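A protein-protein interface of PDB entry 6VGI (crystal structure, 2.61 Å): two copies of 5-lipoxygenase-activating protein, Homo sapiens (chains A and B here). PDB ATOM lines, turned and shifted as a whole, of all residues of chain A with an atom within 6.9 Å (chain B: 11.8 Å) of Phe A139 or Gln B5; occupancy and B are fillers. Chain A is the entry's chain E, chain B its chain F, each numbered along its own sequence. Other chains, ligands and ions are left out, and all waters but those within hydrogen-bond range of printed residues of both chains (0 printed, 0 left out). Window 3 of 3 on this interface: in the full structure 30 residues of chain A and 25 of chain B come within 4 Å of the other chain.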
ATOM      1  N   ASN A 134       7.454 -13.430 -24.459  1.00  0.00           N
ATOM      2  CA  ASN A 134       8.228 -12.729 -23.440  1.00  0.00           C
ATOM      3  C   ASN A 134       7.371 -12.388 -22.224  1.00  0.00           C
ATOM      4  O   ASN A 134       7.848 -12.438 -21.091  1.00  0.00           O
ATOM      5  CB  ASN A 134       8.858 -11.461 -24.022  1.00  0.00           C
ATOM      6  CG  ASN A 134       9.589 -10.636 -22.980  1.00  0.00           C
ATOM      7  OD1 ASN A 134       9.163  -9.533 -22.642  1.00  0.00           O
ATOM      8  ND2 ASN A 134      10.687 -11.173 -22.455  1.00  0.00           N
ATOM      9  N   TYR A 135       6.107 -12.045 -22.471  1.00  0.00           N
ATOM     10  CA  TYR A 135       5.148 -11.770 -21.403  1.00  0.00           C
ATOM     11  C   TYR A 135       4.914 -12.999 -20.528  1.00  0.00           C
ATOM     12  O   TYR A 135       4.960 -12.905 -19.301  1.00  0.00           O
ATOM     13  CB  TYR A 135       3.816 -11.262 -21.976  1.00  0.00           C
ATOM     14  CG  TYR A 135       2.662 -11.318 -20.991  1.00  0.00           C
ATOM     15  CD1 TYR A 135       2.492 -10.322 -20.029  1.00  0.00           C
ATOM     16  CD2 TYR A 135       1.746 -12.373 -21.018  1.00  0.00           C
ATOM     17  CE1 TYR A 135       1.440 -10.371 -19.120  1.00  0.00           C
ATOM     18  CE2 TYR A 135       0.691 -12.432 -20.112  1.00  0.00           C
ATOM     19  CZ  TYR A 135       0.545 -11.427 -19.167  1.00  0.00           C
ATOM     20  OH  TYR A 135      -0.494 -11.476 -18.266  1.00  0.00           O
ATOM     21  N   TYR A 136       4.664 -14.143 -21.163  1.00  0.00           N
ATOM     22  CA  TYR A 136       4.353 -15.381 -20.444  1.00  0.00           C
ATOM     23  C   TYR A 136       5.548 -15.963 -19.695  1.00  0.00           C
ATOM     24  O   TYR A 136       5.370 -16.673 -18.705  1.00  0.00           O
ATOM     25  CB  TYR A 136       3.737 -16.425 -21.384  1.00  0.00           C
ATOM     26  CG  TYR A 136       2.287 -16.147 -21.726  1.00  0.00           C
ATOM     27  CD1 TYR A 136       1.933 -15.601 -22.960  1.00  0.00           C
ATOM     28  CD2 TYR A 136       1.269 -16.423 -20.811  1.00  0.00           C
ATOM     29  CE1 TYR A 136       0.603 -15.341 -23.278  1.00  0.00           C
ATOM     30  CE2 TYR A 136      -0.065 -16.166 -21.118  1.00  0.00           C
ATOM     31  CZ  TYR A 136      -0.391 -15.624 -22.353  1.00  0.00           C
ATOM     32  OH  TYR A 136      -1.709 -15.366 -22.664  1.00  0.00           O
ATOM     33  N   LEU A 137       6.755 -15.660 -20.166  1.00  0.00           N
ATOM     34  CA  LEU A 137       7.979 -16.085 -19.490  1.00  0.00           C
ATOM     35  C   LEU A 137       8.155 -15.382 -18.147  1.00  0.00           C
ATOM     36  O   LEU A 137       8.406 -16.033 -17.134  1.00  0.00           O
ATOM     37  CB  LEU A 137       9.210 -15.850 -20.373  1.00  0.00           C
ATOM     38  CG  LEU A 137       9.639 -16.970 -21.328  1.00  0.00           C
ATOM     39  CD1 LEU A 137      10.678 -16.451 -22.308  1.00  0.00           C
ATOM     40  CD2 LEU A 137      10.175 -18.179 -20.567  1.00  0.00           C
ATOM     41  N   ILE A 138       8.013 -14.059 -18.151  1.00  0.00           N
ATOM     42  CA  ILE A 138       8.153 -13.245 -16.939  1.00  0.00           C
ATOM     43  C   ILE A 138       7.018 -13.532 -15.949  1.00  0.00           C
ATOM     44  O   ILE A 138       7.239 -13.546 -14.735  1.00  0.00           O
ATOM     45  CB  ILE A 138       8.237 -11.725 -17.272  1.00  0.00           C
ATOM     46  CG1 ILE A 138       9.385 -11.452 -18.252  1.00  0.00           C
ATOM     47  CG2 ILE A 138       8.435 -10.895 -16.008  1.00  0.00           C
ATOM     48  CD1 ILE A 138       9.289 -10.116 -18.977  1.00  0.00           C
ATOM     49  N   PHE A 139       5.818 -13.780 -16.478  1.00  0.00           N
ATOM     50  CA  PHE A 139       4.639 -14.086 -15.664  1.00  0.00           C
ATOM     51  C   PHE A 139       4.790 -15.405 -14.903  1.00  0.00           C
ATOM     52  O   PHE A 139       4.546 -15.460 -13.694  1.00  0.00           O
ATOM     53  CB  PHE A 139       3.373 -14.110 -16.532  1.00  0.00           C
ATOM     54  CG  PHE A 139       2.097 -14.280 -15.748  1.00  0.00           C
ATOM     55  CD1 PHE A 139       1.422 -13.171 -15.243  1.00  0.00           C
ATOM     56  CD2 PHE A 139       1.565 -15.549 -15.521  1.00  0.00           C
ATOM     57  CE1 PHE A 139       0.240 -13.321 -14.517  1.00  0.00           C
ATOM     58  CE2 PHE A 139       0.385 -15.711 -14.796  1.00  0.00           C
ATOM     59  CZ  PHE A 139      -0.280 -14.594 -14.294  1.00  0.00           C
ATOM     60  N   PHE A 140       5.185 -16.457 -15.617  1.00  0.00           N
ATOM     61  CA  PHE A 140       5.402 -17.771 -15.011  1.00  0.00           C
ATOM     62  C   PHE A 140       6.585 -17.766 -14.047  1.00  0.00           C
ATOM     63  O   PHE A 140       6.561 -18.463 -13.031  1.00  0.00           O
ATOM     64  CB  PHE A 140       5.579 -18.852 -16.084  1.00  0.00           C
ATOM     65  CG  PHE A 140       4.292 -19.520 -16.491  1.00  0.00           C
ATOM     66  CD1 PHE A 140       3.463 -18.946 -17.454  1.00  0.00           C
ATOM     67  CD2 PHE A 140       3.906 -20.727 -15.910  1.00  0.00           C
ATOM     68  CE1 PHE A 140       2.270 -19.562 -17.832  1.00  0.00           C
ATOM     69  CE2 PHE A 140       2.715 -21.353 -16.280  1.00  0.00           C
ATOM     70  CZ  PHE A 140       1.896 -20.769 -17.244  1.00  0.00           C
ATOM     71  N   PHE A 141       7.606 -16.973 -14.369  1.00  0.00           N
ATOM     72  CA  PHE A 141       8.753 -16.769 -13.486  1.00  0.00           C
ATOM     73  C   PHE A 141       8.324 -16.006 -12.232  1.00  0.00           C
ATOM     74  O   PHE A 141       8.843 -16.249 -11.141  1.00  0.00           O
ATOM     75  CB  PHE A 141       9.867 -16.016 -14.221  1.00  0.00           C
ATOM     76  CG  PHE A 141      11.151 -15.906 -13.443  1.00  0.00           C
ATOM     77  CD1 PHE A 141      12.054 -16.966 -13.406  1.00  0.00           C
ATOM     78  CD2 PHE A 141      11.467 -14.734 -12.759  1.00  0.00           C
ATOM     79  CE1 PHE A 141      13.248 -16.866 -12.690  1.00  0.00           C
ATOM     80  CE2 PHE A 141      12.657 -14.624 -12.041  1.00  0.00           C
ATOM     81  CZ  PHE A 141      13.549 -15.692 -12.007  1.00  0.00           C
ATOM     82  N   GLY A 142       7.371 -15.091 -12.408  1.00  0.00           N
ATOM     83  CA  GLY A 142       6.791 -14.321 -11.311  1.00  0.00           C
ATOM     84  C   GLY A 142       5.965 -15.171 -10.365  1.00  0.00           C
ATOM     85  O   GLY A 142       5.948 -14.925  -9.159  1.00  0.00           O
ATOM     86  N   SER A 143       5.274 -16.167 -10.912  1.00  0.00           N
ATOM     87  CA  SER A 143       4.536 -17.129 -10.099  1.00  0.00           C
ATOM     88  C   SER A 143       5.486 -18.147  -9.468  1.00  0.00           C
ATOM     89  O   SER A 143       5.243 -18.612  -8.355  1.00  0.00           O
ATOM     90  CB  SER A 143       3.455 -17.831 -10.923  1.00  0.00           C
ATOM     91  OG  SER A 143       4.020 -18.550 -12.003  1.00  0.00           O
ATOM     92  N   ASP A 144       6.561 -18.481 -10.181  1.00  0.00           N
ATOM     93  CA  ASP A 144       7.605 -19.371  -9.665  1.00  0.00           C
ATOM     94  C   ASP A 144       8.328 -18.769  -8.465  1.00  0.00           C
ATOM     95  O   ASP A 144       8.666 -19.480  -7.521  1.00  0.00           O
ATOM     96  CB  ASP A 144       8.620 -19.717 -10.760  1.00  0.00           C
ATOM     97  CG  ASP A 144       8.238 -20.962 -11.549  1.00  0.00           C
ATOM     98  OD1 ASP A 144       7.047 -21.130 -11.890  1.00  0.00           O
ATOM     99  OD2 ASP A 144       9.143 -21.774 -11.837  1.00  0.00           O
ATOM    100  N   PHE A 145       8.567 -17.460  -8.517  1.00  0.00           N
ATOM    101  CA  PHE A 145       9.162 -16.728  -7.404  1.00  0.00           C
ATOM    102  C   PHE A 145       8.179 -16.645  -6.239  1.00  0.00           C
ATOM    103  O   PHE A 145       8.552 -16.881  -5.091  1.00  0.00           O
ATOM    104  CB  PHE A 145       9.590 -15.325  -7.851  1.00  0.00           C
ATOM    105  CG  PHE A 145      10.295 -14.527  -6.783  1.00  0.00           C
ATOM    106  CD1 PHE A 145      11.640 -14.755  -6.495  1.00  0.00           C
ATOM    107  CD2 PHE A 145       9.618 -13.538  -6.073  1.00  0.00           C
ATOM    108  CE1 PHE A 145      12.296 -14.016  -5.510  1.00  0.00           C
ATOM    109  CE2 PHE A 145      10.264 -12.793  -5.088  1.00  0.00           C
ATOM    110  CZ  PHE A 145      11.606 -13.033  -4.806  1.00  0.00           C
ATOM    111  N   SER B   2       8.645  -2.994 -23.812  1.00  0.00           N
ATOM    112  CA  SER B   2       8.666  -1.582 -23.327  1.00  0.00           C
ATOM    113  C   SER B   2       7.601  -1.333 -22.257  1.00  0.00           C
ATOM    114  O   SER B   2       7.887  -0.728 -21.221  1.00  0.00           O
ATOM    115  CB  SER B   2       8.485  -0.606 -24.497  1.00  0.00           C
ATOM    116  OG  SER B   2       9.526  -0.745 -25.450  1.00  0.00           O
ATOM    117  N   LEU B   3       6.383  -1.804 -22.518  1.00  0.00           N
ATOM    118  CA  LEU B   3       5.255  -1.642 -21.597  1.00  0.00           C
ATOM    119  C   LEU B   3       5.345  -2.582 -20.396  1.00  0.00           C
ATOM    120  O   LEU B   3       6.039  -3.601 -20.445  1.00  0.00           O
ATOM    121  CB  LEU B   3       3.923  -1.849 -22.331  1.00  0.00           C
ATOM    122  CG  LEU B   3       3.329  -0.680 -23.123  1.00  0.00           C
ATOM    123  CD1 LEU B   3       4.106  -0.406 -24.407  1.00  0.00           C
ATOM    124  CD2 LEU B   3       1.864  -0.950 -23.438  1.00  0.00           C
ATOM    125  N   ASP B   4       4.632  -2.232 -19.326  1.00  0.00           N
ATOM    126  CA  ASP B   4       4.640  -3.005 -18.081  1.00  0.00           C
ATOM    127  C   ASP B   4       3.899  -4.340 -18.193  1.00  0.00           C
ATOM    128  O   ASP B   4       3.143  -4.566 -19.138  1.00  0.00           O
ATOM    129  CB  ASP B   4       4.076  -2.170 -16.921  1.00  0.00           C
ATOM    130  CG  ASP B   4       2.663  -1.678 -17.180  1.00  0.00           C
ATOM    131  OD1 ASP B   4       1.752  -2.070 -16.420  1.00  0.00           O
ATOM    132  OD2 ASP B   4       2.462  -0.903 -18.141  1.00  0.00           O
ATOM    133  N   GLN B   5       4.122  -5.212 -17.213  1.00  0.00           N
ATOM    134  CA  GLN B   5       3.546  -6.556 -17.194  1.00  0.00           C
ATOM    135  C   GLN B   5       2.048  -6.556 -16.881  1.00  0.00           C
ATOM    136  O   GLN B   5       1.327  -7.476 -17.273  1.00  0.00           O
ATOM    137  CB  GLN B   5       4.302  -7.432 -16.185  1.00  0.00           C
ATOM    138  CG  GLN B   5       3.989  -8.932 -16.247  1.00  0.00           C
ATOM    139  CD  GLN B   5       4.691  -9.660 -17.390  1.00  0.00           C
ATOM    140  OE1 GLN B   5       5.271  -9.045 -18.288  1.00  0.00           O
ATOM    141  NE2 GLN B   5       4.635 -10.985 -17.357  1.00  0.00           N
ATOM    142  N   GLU B   6       1.584  -5.519 -16.186  1.00  0.00           N
ATOM    143  CA  GLU B   6       0.199  -5.453 -15.721  1.00  0.00           C
ATOM    144  C   GLU B   6      -0.784  -5.173 -16.858  1.00  0.00           C
ATOM    145  O   GLU B   6      -1.756  -5.913 -17.042  1.00  0.00           O
ATOM    146  CB  GLU B   6       0.054  -4.402 -14.614  1.00  0.00           C
ATOM    147  CG  GLU B   6      -0.715  -4.882 -13.385  1.00  0.00           C
ATOM    148  CD  GLU B   6      -2.142  -5.312 -13.688  1.00  0.00           C
ATOM    149  OE1 GLU B   6      -2.914  -4.495 -14.235  1.00  0.00           O
ATOM    150  OE2 GLU B   6      -2.494  -6.465 -13.363  1.00  0.00           O
ATOM    151  N   THR B   7      -0.521  -4.111 -17.619  1.00  0.00           N
ATOM    152  CA  THR B   7      -1.401  -3.684 -18.711  1.00  0.00           C
ATOM    153  C   THR B   7      -1.363  -4.609 -19.931  1.00  0.00           C
ATOM    154  O   THR B   7      -2.331  -4.670 -20.694  1.00  0.00           O
ATOM    155  CB  THR B   7      -1.110  -2.232 -19.156  1.00  0.00           C
ATOM    156  OG1 THR B   7       0.304  -2.039 -19.278  1.00  0.00           O
ATOM    157  CG2 THR B   7      -1.671  -1.235 -18.149  1.00  0.00           C
ATOM    158  N   VAL B   8      -0.252  -5.322 -20.114  1.00  0.00           N
ATOM    159  CA  VAL B   8      -0.130  -6.304 -21.198  1.00  0.00           C
ATOM    160  C   VAL B   8      -0.993  -7.539 -20.904  1.00  0.00           C
ATOM    161  O   VAL B   8      -1.451  -8.217 -21.823  1.00  0.00           O
ATOM    162  CB  VAL B   8       1.354  -6.673 -21.496  1.00  0.00           C
ATOM    163  CG1 VAL B   8       1.459  -7.865 -22.443  1.00  0.00           C
ATOM    164  CG2 VAL B   8       2.082  -5.478 -22.097  1.00  0.00           C
ATOM    165  N   GLY B   9      -1.231  -7.804 -19.622  1.00  0.00           N
ATOM    166  CA  GLY B   9      -2.142  -8.870 -19.205  1.00  0.00           C
ATOM    167  C   GLY B   9      -3.601  -8.536 -19.466  1.00  0.00           C
ATOM    168  O   GLY B   9      -4.461  -9.419 -19.440  1.00  0.00           O
ATOM    169  N   ASN B  10      -3.877  -7.256 -19.710  1.00  0.00           N
ATOM    170  CA  ASN B  10      -5.226  -6.792 -20.028  1.00  0.00           C
ATOM    171  C   ASN B  10      -5.524  -6.811 -21.527  1.00  0.00           C
ATOM    172  O   ASN B  10      -6.671  -6.615 -21.938  1.00  0.00           O
ATOM    173  CB  ASN B  10      -5.458  -5.382 -19.467  1.00  0.00           C
ATOM    174  CG  ASN B  10      -5.534  -5.355 -17.949  1.00  0.00           C
ATOM    175  OD1 ASN B  10      -5.938  -6.331 -17.314  1.00  0.00           O
ATOM    176  ND2 ASN B  10      -5.150  -4.228 -17.359  1.00  0.00           N
ATOM    177  N   VAL B  11      -4.491  -7.051 -22.334  1.00  0.00           N
ATOM    178  CA  VAL B  11      -4.611  -6.994 -23.794  1.00  0.00           C
ATOM    179  C   VAL B  11      -4.167  -8.279 -24.504  1.00  0.00           C
ATOM    180  O   VAL B  11      -4.482  -8.474 -25.678  1.00  0.00           O
ATOM    181  CB  VAL B  11      -3.834  -5.781 -24.394  1.00  0.00           C
ATOM    182  CG1 VAL B  11      -4.361  -4.462 -23.842  1.00  0.00           C
ATOM    183  CG2 VAL B  11      -2.332  -5.904 -24.149  1.00  0.00           C
ATOM    184  N   VAL B  12      -3.448  -9.144 -23.790  1.00  0.00           N
ATOM    185  CA  VAL B  12      -2.786 -10.315 -24.388  1.00  0.00           C
ATOM    186  C   VAL B  12      -3.726 -11.226 -25.199  1.00  0.00           C
ATOM    187  O   VAL B  12      -3.383 -11.634 -26.311  1.00  0.00           O
ATOM    188  CB  VAL B  12      -1.947 -11.122 -23.335  1.00  0.00           C
ATOM    189  CG1 VAL B  12      -2.834 -11.772 -22.272  1.00  0.00           C
ATOM    190  CG2 VAL B  12      -1.055 -12.157 -24.016  1.00  0.00           C
ATOM    191  N   LEU B  13      -4.904 -11.522 -24.648  1.00  0.00           N
ATOM    192  CA  LEU B  13      -5.894 -12.356 -25.337  1.00  0.00           C
ATOM    193  C   LEU B  13      -6.474 -11.657 -26.563  1.00  0.00           C
ATOM    194  O   LEU B  13      -6.728 -12.300 -27.585  1.00  0.00           O
ATOM    195  CB  LEU B  13      -7.016 -12.791 -24.386  1.00  0.00           C
ATOM    196  CG  LEU B  13      -6.689 -13.817 -23.294  1.00  0.00           C
ATOM    197  CD1 LEU B  13      -7.917 -14.067 -22.433  1.00  0.00           C
ATOM    198  CD2 LEU B  13      -6.170 -15.131 -23.879  1.00  0.00           C
ATOM    199  N   ALA B  15      -4.789  -9.361 -28.216  1.00  0.00           N
ATOM    200  CA  ALA B  15      -3.645  -9.321 -29.122  1.00  0.00           C
ATOM    201  C   ALA B  15      -3.496 -10.619 -29.912  1.00  0.00           C
ATOM    202  O   ALA B  15      -3.186 -10.585 -31.103  1.00  0.00           O
ATOM    203  CB  ALA B  15      -2.366  -9.011 -28.352  1.00  0.00           C
ATOM    204  N   GLN B  82     -12.150  -8.599 -20.923  1.00  0.00           N
ATOM    205  CA  GLN B  82     -11.274  -9.119 -21.978  1.00  0.00           C
ATOM    206  C   GLN B  82     -11.676 -10.496 -22.515  1.00  0.00           C
ATOM    207  O   GLN B  82     -11.795 -10.675 -23.729  1.00  0.00           O
ATOM    208  CB  GLN B  82      -9.813  -9.141 -21.505  1.00  0.00           C
ATOM    209  CG  GLN B  82      -8.802  -9.521 -22.590  1.00  0.00           C
ATOM    210  CD  GLN B  82      -7.377  -9.672 -22.075  1.00  0.00           C
ATOM    211  OE1 GLN B  82      -6.450  -9.899 -22.853  1.00  0.00           O
ATOM    212  NE2 GLN B  82      -7.195  -9.543 -20.763  1.00  0.00           N
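The side-chain amide nitrogen (NE2) of Gln B5 sits close to the backbone NH (N) of Phe A139 (3.2 Å). The side-chain amide nitrogen (NE2) of Gln B5 lies within hydrogen-bond range of the backbone carbonyl oxygen (O) of Tyr A135, at 2.8 Å.
O of Gly B9 is in hydrogen-bond range of NE2 of Gln B82, at 3.0 Å. The backbone NH of Val B12 sits at hydrogen-bond distance from the side-chain amide oxygen of Gln B82.
Tyr A135 touches Val B8 (CD1 to CG1, 3.6 Å). Tyr A135 touches Gly B9. Val B12 touches Tyr A136. CB of Ile A138 touches NE2 of Gln B5 (3.7 Å).
Phe A139 touches one residue of chain B. Of chain A, only Tyr A135 (2.8 Å), Ile A138 (3.7 Å) and Phe A139 (3.2 Å) come within 4 Å of Gln B5. Tyr A135 touches just these residues of chain B: Gln B5 (2.8 Å), Val B8 (3.6 Å) and Gly B9 (3.2 Å). Ile A138 touches one residue of chain B. No residue of chain B comes within 4 Å of Phe A140. No residue of chain B comes within 4 Å of Gly A142. No residue of chain B comes within 4 Å of Ser A143. Printed residues of chain A within 4 Å of Val B8: Tyr A135. Printed residues of chain A within 4 Å of Val B12: Tyr A136 (3.5 Å). Of the printed residues of chain A, Gly B9 touches Tyr A135 (3.2 Å). Of the printed residues of chain B, Tyr A136 touches Val B12. Leu A137 touches none of the printed residues of chain B. Ser B2 touches none of the printed residues of chain A. The nearest printed residue of chain A that does not touch Gly B9 is Phe A139 (6.8 Å).
Hydrophobic or aromatic side chains of chain A that line the printed part of chain B: Tyr A135, Tyr A136, Ile A138 and Phe A139. Among the printed residues, no Asp or Glu carboxylate lies within 4 Å of a Lys or Arg side-chain nitrogen of the other chain.
No position is printed for both chains.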
